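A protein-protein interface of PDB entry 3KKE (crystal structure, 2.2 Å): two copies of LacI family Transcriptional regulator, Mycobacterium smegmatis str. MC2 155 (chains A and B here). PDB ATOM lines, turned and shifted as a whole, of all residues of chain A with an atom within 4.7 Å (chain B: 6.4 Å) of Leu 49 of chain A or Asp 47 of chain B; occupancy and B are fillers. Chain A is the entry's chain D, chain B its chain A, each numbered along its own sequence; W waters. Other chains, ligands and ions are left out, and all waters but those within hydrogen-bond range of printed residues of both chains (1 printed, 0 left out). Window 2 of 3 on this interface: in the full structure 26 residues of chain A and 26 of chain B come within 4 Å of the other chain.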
ATOM      1  N   THR A  17      -2.905   0.226  17.592  1.00  0.00           N
ATOM      2  CA  THR A  17      -3.764  -0.364  18.648  1.00  0.00           C
ATOM      3  C   THR A  17      -3.026  -1.487  19.402  1.00  0.00           C
ATOM      4  O   THR A  17      -2.384  -2.335  18.782  1.00  0.00           O
ATOM      5  CB  THR A  17      -5.092  -0.959  18.053  1.00  0.00           C
ATOM      6  OG1 THR A  17      -5.851   0.045  17.348  1.00  0.00           O
ATOM      7  CG2 THR A  17      -5.961  -1.540  19.159  1.00  0.00           C
ATOM      8  N   ILE A  18      -3.118  -1.491  20.735  1.00  0.00           N
ATOM      9  CA  ILE A  18      -2.651  -2.624  21.547  1.00  0.00           C
ATOM     10  C   ILE A  18      -3.791  -3.282  22.319  1.00  0.00           C
ATOM     11  O   ILE A  18      -4.797  -2.643  22.629  1.00  0.00           O
ATOM     12  CB  ILE A  18      -1.528  -2.236  22.565  1.00  0.00           C
ATOM     13  CG1 ILE A  18      -2.064  -1.350  23.684  1.00  0.00           C
ATOM     14  CG2 ILE A  18      -0.316  -1.542  21.862  1.00  0.00           C
ATOM     15  CD1 ILE A  18      -1.007  -1.028  24.721  1.00  0.00           C
ATOM     16  N   GLY A  19      -3.612  -4.560  22.625  1.00  0.00           N
ATOM     17  CA  GLY A  19      -4.577  -5.344  23.362  1.00  0.00           C
ATOM     18  C   GLY A  19      -4.312  -5.338  24.855  1.00  0.00           C
ATOM     19  O   GLY A  19      -3.189  -5.506  25.285  1.00  0.00           O
ATOM     20  N   LEU A  20      -5.330  -5.113  25.670  1.00  0.00           N
ATOM     21  CA  LEU A  20      -5.185  -5.332  27.093  1.00  0.00           C
ATOM     22  C   LEU A  20      -6.085  -6.497  27.367  1.00  0.00           C
ATOM     23  O   LEU A  20      -7.316  -6.374  27.273  1.00  0.00           O
ATOM     24  CB  LEU A  20      -5.566  -4.092  27.893  1.00  0.00           C
ATOM     25  CG  LEU A  20      -5.673  -4.232  29.406  1.00  0.00           C
ATOM     26  CD1 LEU A  20      -4.343  -4.687  30.021  1.00  0.00           C
ATOM     27  CD2 LEU A  20      -6.100  -2.917  30.024  1.00  0.00           C
ATOM     28  N   ASP A  47      -4.398   3.280  20.626  1.00  0.00           N
ATOM     29  CA  ASP A  47      -5.677   2.869  21.174  1.00  0.00           C
ATOM     30  C   ASP A  47      -5.531   1.546  21.897  1.00  0.00           C
ATOM     31  O   ASP A  47      -4.607   0.754  21.612  1.00  0.00           O
ATOM     32  CB  ASP A  47      -6.704   2.745  20.054  1.00  0.00           C
ATOM     33  CG  ASP A  47      -6.995   4.083  19.381  1.00  0.00           C
ATOM     34  OD1 ASP A  47      -6.956   4.158  18.133  1.00  0.00           O
ATOM     35  OD2 ASP A  47      -7.238   5.067  20.108  1.00  0.00           O
ATOM     36  N   VAL A  48      -6.440   1.316  22.845  1.00  0.00           N
ATOM     37  CA  VAL A  48      -6.412   0.117  23.658  1.00  0.00           C
ATOM     38  C   VAL A  48      -7.630  -0.721  23.356  1.00  0.00           C
ATOM     39  O   VAL A  48      -8.775  -0.232  23.383  1.00  0.00           O
ATOM     40  CB  VAL A  48      -6.377   0.448  25.153  1.00  0.00           C
ATOM     41  CG1 VAL A  48      -6.278  -0.837  25.983  1.00  0.00           C
ATOM     42  CG2 VAL A  48      -5.246   1.406  25.454  1.00  0.00           C
ATOM     43  N   LEU A  49      -7.391  -1.983  23.060  1.00  0.00           N
ATOM     44  CA  LEU A  49      -8.467  -2.903  22.815  1.00  0.00           C
ATOM     45  C   LEU A  49      -8.531  -3.830  23.990  1.00  0.00           C
ATOM     46  O   LEU A  49      -7.530  -4.431  24.346  1.00  0.00           O
ATOM     47  CB  LEU A  49      -8.239  -3.669  21.537  1.00  0.00           C
ATOM     48  CG  LEU A  49      -9.182  -4.836  21.286  1.00  0.00           C
ATOM     49  CD1 LEU A  49      -9.008  -5.304  19.855  1.00  0.00           C
ATOM     50  CD2 LEU A  49      -9.008  -5.979  22.323  1.00  0.00           C
ATOM     51  N   LEU A  50      -9.708  -3.938  24.599  1.00  0.00           N
ATOM     52  CA  LEU A  50      -9.877  -4.726  25.811  1.00  0.00           C
ATOM     53  C   LEU A  50     -10.465  -6.078  25.446  1.00  0.00           C
ATOM     54  O   LEU A  50     -11.500  -6.166  24.750  1.00  0.00           O
ATOM     55  CB  LEU A  50     -10.768  -3.969  26.793  1.00  0.00           C
ATOM     56  CG  LEU A  50     -10.953  -4.497  28.213  1.00  0.00           C
ATOM     57  CD1 LEU A  50      -9.715  -4.306  29.053  1.00  0.00           C
ATOM     58  CD2 LEU A  50     -12.135  -3.776  28.852  1.00  0.00           C
ATOM     59  N   GLY A  51      -9.810  -7.136  25.899  1.00  0.00           N
ATOM     60  CA  GLY A  51     -10.176  -8.477  25.473  1.00  0.00           C
ATOM     61  C   GLY A  51     -10.048  -9.496  26.573  1.00  0.00           C
ATOM     62  O   GLY A  51      -9.539  -9.200  27.650  1.00  0.00           O
ATOM     63  N   LEU A  66      -5.791 -12.308  16.714  1.00  0.00           N
ATOM     64  CA  LEU A  66      -5.835 -10.884  17.057  1.00  0.00           C
ATOM     65  C   LEU A  66      -4.701 -10.129  16.377  1.00  0.00           C
ATOM     66  O   LEU A  66      -4.921  -9.056  15.820  1.00  0.00           O
ATOM     67  CB  LEU A  66      -5.731 -10.677  18.567  1.00  0.00           C
ATOM     68  CG  LEU A  66      -6.592  -9.559  19.129  1.00  0.00           C
ATOM     69  CD1 LEU A  66      -8.081  -9.965  19.075  1.00  0.00           C
ATOM     70  CD2 LEU A  66      -6.154  -9.219  20.538  1.00  0.00           C
ATOM     71  N   ARG A  71      -5.587  -6.911  14.210  1.00  0.00           N
ATOM     72  CA  ARG A  71      -6.503  -6.233  15.142  1.00  0.00           C
ATOM     73  C   ARG A  71      -5.750  -5.471  16.255  1.00  0.00           C
ATOM     74  O   ARG A  71      -6.188  -4.402  16.689  1.00  0.00           O
ATOM     75  CB  ARG A  71      -7.505  -7.225  15.747  1.00  0.00           C
ATOM     76  CG  ARG A  71      -8.463  -7.884  14.746  1.00  0.00           C
ATOM     77  CD  ARG A  71      -9.401  -8.831  15.498  1.00  0.00           C
ATOM     78  NE  ARG A  71     -10.420  -9.470  14.657  1.00  0.00           N
ATOM     79  CZ  ARG A  71     -11.528  -8.886  14.182  1.00  0.00           C
ATOM     80  NH1 ARG A  71     -11.795  -7.607  14.418  1.00  0.00           N
ATOM     81  NH2 ARG A  71     -12.376  -9.585  13.440  1.00  0.00           N
ATOM     82  N   VAL A  72      -4.632  -6.043  16.709  1.00  0.00           N
ATOM     83  CA  VAL A  72      -3.678  -5.386  17.628  1.00  0.00           C
ATOM     84  C   VAL A  72      -2.225  -5.517  17.131  1.00  0.00           C
ATOM     85  O   VAL A  72      -1.895  -6.484  16.460  1.00  0.00           O
ATOM     86  CB  VAL A  72      -3.731  -6.002  19.034  1.00  0.00           C
ATOM     87  CG1 VAL A  72      -5.138  -5.912  19.605  1.00  0.00           C
ATOM     88  CG2 VAL A  72      -3.257  -7.445  18.999  1.00  0.00           C
ATOM     89  N   THR B  17     -14.817  -1.964  13.697  1.00  0.00           N
ATOM     90  CA  THR B  17     -14.496  -1.691  15.136  1.00  0.00           C
ATOM     91  C   THR B  17     -15.351  -0.568  15.770  1.00  0.00           C
ATOM     92  O   THR B  17     -15.694   0.417  15.107  1.00  0.00           O
ATOM     93  CB  THR B  17     -13.006  -1.342  15.321  1.00  0.00           C
ATOM     94  OG1 THR B  17     -12.790   0.058  15.094  1.00  0.00           O
ATOM     95  CG2 THR B  17     -12.125  -2.157  14.365  1.00  0.00           C
ATOM     96  N   ILE B  18     -15.685  -0.731  17.053  1.00  0.00           N
ATOM     97  CA  ILE B  18     -16.441   0.279  17.812  1.00  0.00           C
ATOM     98  C   ILE B  18     -15.705   0.761  19.069  1.00  0.00           C
ATOM     99  O   ILE B  18     -14.838   0.074  19.608  1.00  0.00           O
ATOM    100  CB  ILE B  18     -17.871  -0.214  18.215  1.00  0.00           C
ATOM    101  CG1 ILE B  18     -17.810  -1.423  19.139  1.00  0.00           C
ATOM    102  CG2 ILE B  18     -18.696  -0.528  16.983  1.00  0.00           C
ATOM    103  CD1 ILE B  18     -19.156  -1.997  19.483  1.00  0.00           C
ATOM    104  N   GLY B  19     -16.039   1.983  19.496  1.00  0.00           N
ATOM    105  CA  GLY B  19     -15.450   2.608  20.690  1.00  0.00           C
ATOM    106  C   GLY B  19     -16.455   2.619  21.841  1.00  0.00           C
ATOM    107  O   GLY B  19     -17.623   2.962  21.656  1.00  0.00           O
ATOM    108  N   GLN B  38     -19.275  -6.578  24.591  1.00  0.00           N
ATOM    109  CA  GLN B  38     -18.237  -7.422  24.030  1.00  0.00           C
ATOM    110  C   GLN B  38     -18.815  -8.657  23.348  1.00  0.00           C
ATOM    111  O   GLN B  38     -18.425  -8.982  22.215  1.00  0.00           O
ATOM    112  CB  GLN B  38     -17.209  -7.819  25.104  1.00  0.00           C
ATOM    113  CG  GLN B  38     -15.972  -8.523  24.508  1.00  0.00           C
ATOM    114  CD  GLN B  38     -14.934  -8.928  25.564  1.00  0.00           C
ATOM    115  OE1 GLN B  38     -15.167  -9.859  26.341  1.00  0.00           O
ATOM    116  NE2 GLN B  38     -13.774  -8.259  25.561  1.00  0.00           N
ATOM    117  N   ALA B  41     -20.605  -7.462  20.044  1.00  0.00           N
ATOM    118  CA  ALA B  41     -19.610  -6.967  19.122  1.00  0.00           C
ATOM    119  C   ALA B  41     -18.763  -8.148  18.556  1.00  0.00           C
ATOM    120  O   ALA B  41     -18.645  -8.285  17.342  1.00  0.00           O
ATOM    121  CB  ALA B  41     -18.728  -5.952  19.821  1.00  0.00           C
ATOM    122  N   SER B  42     -18.274  -9.027  19.428  1.00  0.00           N
ATOM    123  CA  SER B  42     -17.449 -10.173  18.983  1.00  0.00           C
ATOM    124  C   SER B  42     -18.250 -11.098  18.096  1.00  0.00           C
ATOM    125  O   SER B  42     -17.692 -11.744  17.184  1.00  0.00           O
ATOM    126  CB  SER B  42     -16.900 -10.980  20.161  1.00  0.00           C
ATOM    127  OG  SER B  42     -15.971 -10.192  20.878  1.00  0.00           O
ATOM    128  N   SER B  45     -17.679 -10.184  14.771  1.00  0.00           N
ATOM    129  CA  SER B  45     -16.239  -9.998  14.485  1.00  0.00           C
ATOM    130  C   SER B  45     -15.835  -8.514  14.539  1.00  0.00           C
ATOM    131  O   SER B  45     -15.054  -8.048  13.722  1.00  0.00           O
ATOM    132  CB  SER B  45     -15.901 -10.618  13.123  1.00  0.00           C
ATOM    133  OG  SER B  45     -16.249 -11.992  13.103  1.00  0.00           O
ATOM    134  N   THR B  46     -16.393  -7.779  15.504  1.00  0.00           N
ATOM    135  CA  THR B  46     -16.081  -6.350  15.687  1.00  0.00           C
ATOM    136  C   THR B  46     -15.392  -6.146  17.038  1.00  0.00           C
ATOM    137  O   THR B  46     -15.811  -6.699  18.056  1.00  0.00           O
ATOM    138  CB  THR B  46     -17.372  -5.507  15.631  1.00  0.00           C
ATOM    139  OG1 THR B  46     -17.872  -5.511  14.298  1.00  0.00           O
ATOM    140  CG2 THR B  46     -17.130  -4.072  16.077  1.00  0.00           C
ATOM    141  N   ASP B  47     -14.327  -5.367  17.057  1.00  0.00           N
ATOM    142  CA  ASP B  47     -13.582  -5.193  18.284  1.00  0.00           C
ATOM    143  C   ASP B  47     -14.051  -3.932  18.992  1.00  0.00           C
ATOM    144  O   ASP B  47     -14.531  -2.983  18.348  1.00  0.00           O
ATOM    145  CB  ASP B  47     -12.101  -5.054  18.005  1.00  0.00           C
ATOM    146  CG  ASP B  47     -11.507  -6.282  17.349  1.00  0.00           C
ATOM    147  OD1 ASP B  47     -10.903  -6.119  16.265  1.00  0.00           O
ATOM    148  OD2 ASP B  47     -11.639  -7.403  17.898  1.00  0.00           O
ATOM    149  N   VAL B  48     -13.827  -3.934  20.308  1.00  0.00           N
ATOM    150  CA  VAL B  48     -14.200  -2.874  21.190  1.00  0.00           C
ATOM    151  C   VAL B  48     -12.961  -2.184  21.761  1.00  0.00           C
ATOM    152  O   VAL B  48     -12.113  -2.784  22.425  1.00  0.00           O
ATOM    153  CB  VAL B  48     -15.133  -3.410  22.320  1.00  0.00           C
ATOM    154  CG1 VAL B  48     -15.494  -2.299  23.305  1.00  0.00           C
ATOM    155  CG2 VAL B  48     -16.353  -4.074  21.724  1.00  0.00           C
ATOM    156  N   LEU B  49     -12.896  -0.893  21.491  1.00  0.00           N
ATOM    157  CA  LEU B  49     -11.820  -0.017  21.872  1.00  0.00           C
ATOM    158  C   LEU B  49     -12.338   0.817  23.032  1.00  0.00           C
ATOM    159  O   LEU B  49     -13.358   1.506  22.919  1.00  0.00           O
ATOM    160  CB  LEU B  49     -11.523   0.903  20.703  1.00  0.00           C
ATOM    161  CG  LEU B  49     -10.128   0.992  20.165  1.00  0.00           C
ATOM    162  CD1 LEU B  49      -9.800  -0.245  19.323  1.00  0.00           C
ATOM    163  CD2 LEU B  49      -9.990   2.275  19.335  1.00  0.00           C
ATOM    164  N   LEU B  50     -11.652   0.761  24.156  1.00  0.00           N
ATOM    165  CA  LEU B  50     -12.174   1.323  25.374  1.00  0.00           C
ATOM    166  C   LEU B  50     -11.520   2.644  25.669  1.00  0.00           C
ATOM    167  O   LEU B  50     -10.327   2.777  25.564  1.00  0.00           O
ATOM    168  CB  LEU B  50     -11.966   0.347  26.520  1.00  0.00           C
ATOM    169  CG  LEU B  50     -12.435   0.881  27.871  1.00  0.00           C
ATOM    170  CD1 LEU B  50     -13.971   1.076  27.886  1.00  0.00           C
ATOM    171  CD2 LEU B  50     -11.949  -0.051  29.022  1.00  0.00           C
HETATM  172  O   HOH W   1     -13.015  -6.215  21.751  1.00  0.00           O
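Of chain B, only Asp 47 (3.6 Å) and Val 48 (3.7 Å) come within 4 Å of Leu 49 of chain A.
Of the printed residues of chain B, Arg 71 of chain A touches Ser 45 and Asp 47.
Val 72 of chain A touches none of the printed residues of chain B.
Ile 18 of chain B touches none of the printed residues of chain A.
Of the printed residues of chain A, Ser 45 of chain B touches Arg 71 (3.1 Å).
Asp 47 of chain B touches two residues of chain A.
Of the printed residues of chain A, Val 48 of chain B touches Leu 49 and Leu 50.
The nearest residue of chain B that does not touch Leu 49 of chain A is Leu 49 of chain B (4.4 Å).
The nearest printed residue of chain B that does not touch Leu 50 of chain A is Leu 49 of chain B (5.2 Å).
CB of Asp 47 of chain A touches CD2 of Leu 49 of chain B, at 3.4 Å.
Val 48 of chain A touches Leu 49 of chain B (O to CA, 3.4 Å).
Asp 47 of chain B touches Leu 49 of chain A.
CA of Leu 49 of chain A touches O of Val 48 of chain B (3.7 Å).
CD2 of Leu 50 of chain A touches CD2 of Leu 50 of chain B, 3.7 Å away.
NE2 of Gln 38 of chain B touches CA of Gly 51 of chain A, 3.6 Å away.
Water W1 lies within hydrogen-bond range of the backbone NH (N) of Val 48 of chain B (2.8 Å) and the backbone carbonyl oxygen (O) of Leu 50 of chain A (3.4 Å).
The backbone NH (N) of Ile 18 of chain B sits at hydrogen-bond distance from the backbone carbonyl oxygen (O) of Asp 47 of chain B, at 2.8 Å.
The backbone carbonyl oxygen (O) of Ile 18 of chain B sits at hydrogen-bond distance from the backbone NH (N) of Leu 49 of chain B, at 2.9 Å.
OG of Ser 42 of chain B is in hydrogen-bond range of O of Gln 38 of chain B (3.0 Å).
O of Asp 47 of chain A lies within hydrogen-bond range of N of Ile 18 of chain A (2.8 Å).
The backbone NH (N) of Gly 51 of chain A sits at hydrogen-bond distance from the backbone carbonyl oxygen (O) of Leu 20 of chain A, at 2.9 Å.
The backbone carbonyl oxygen of Leu 66 of chain A lies within hydrogen-bond range of the backbone NH of Arg 71 of chain A, 2.8 Å away.
Asp 47 of chain A touches Leu 49 of chain B, and with the chains exchanged Leu 49 of chain A touches Asp 47 of chain B.
Val 48 of chain A touches Leu 49 of chain B, and with the chains exchanged Leu 49 of chain A touches Val 48 of chain B.
Val 48 of chain A touches Leu 50 of chain B, and with the chains exchanged Leu 50 of chain A touches Val 48 of chain B.
Leu 50 of chain B touches its own counterpart, Leu 50 of chain A.
Positions printed for both chains: 17, 18, 19, 47, 48, 49 and 50.
Of the 12 printed residues of chain A, 6 touch a printed residue of chain B.
Printed residues of chain A that touch a printed residue of chain B: Asp 47, Val 48, Leu 49, Leu 50, Gly 51 and Arg 71.
Of the 12 printed residues of chain B, 6 touch a printed residue of chain A.
Hydrophobic or aromatic side chains of chain B that line the printed part of chain A: Leu 49 and Leu 50.
Along chain B the printed residues that touch a printed residue of chain A span positions 38 to 50.
The side-chain amide nitrogen of Gln 38 of chain B is in hydrogen-bond range of the backbone carbonyl oxygen of Leu 50 of chain A, 3.2 Å away.
The backbone carbonyl oxygen of Ser 45 of chain B is in hydrogen-bond range of the guanidinium group of Arg 71 of chain A (3.1 Å).
NH1 of Arg 71 of chain A lies within salt-bridge range of OD1 of Asp 47 of chain B.
The backbone NH (N) of Leu 50 of chain A sits at hydrogen-bond distance from the backbone carbonyl oxygen (O) of Val 48 of chain B, at 3.4 Å.
The backbone carbonyl oxygen (O) of Val 48 of chain A is in hydrogen-bond range of the backbone NH (N) of Leu 50 of chain B (3.1 Å).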
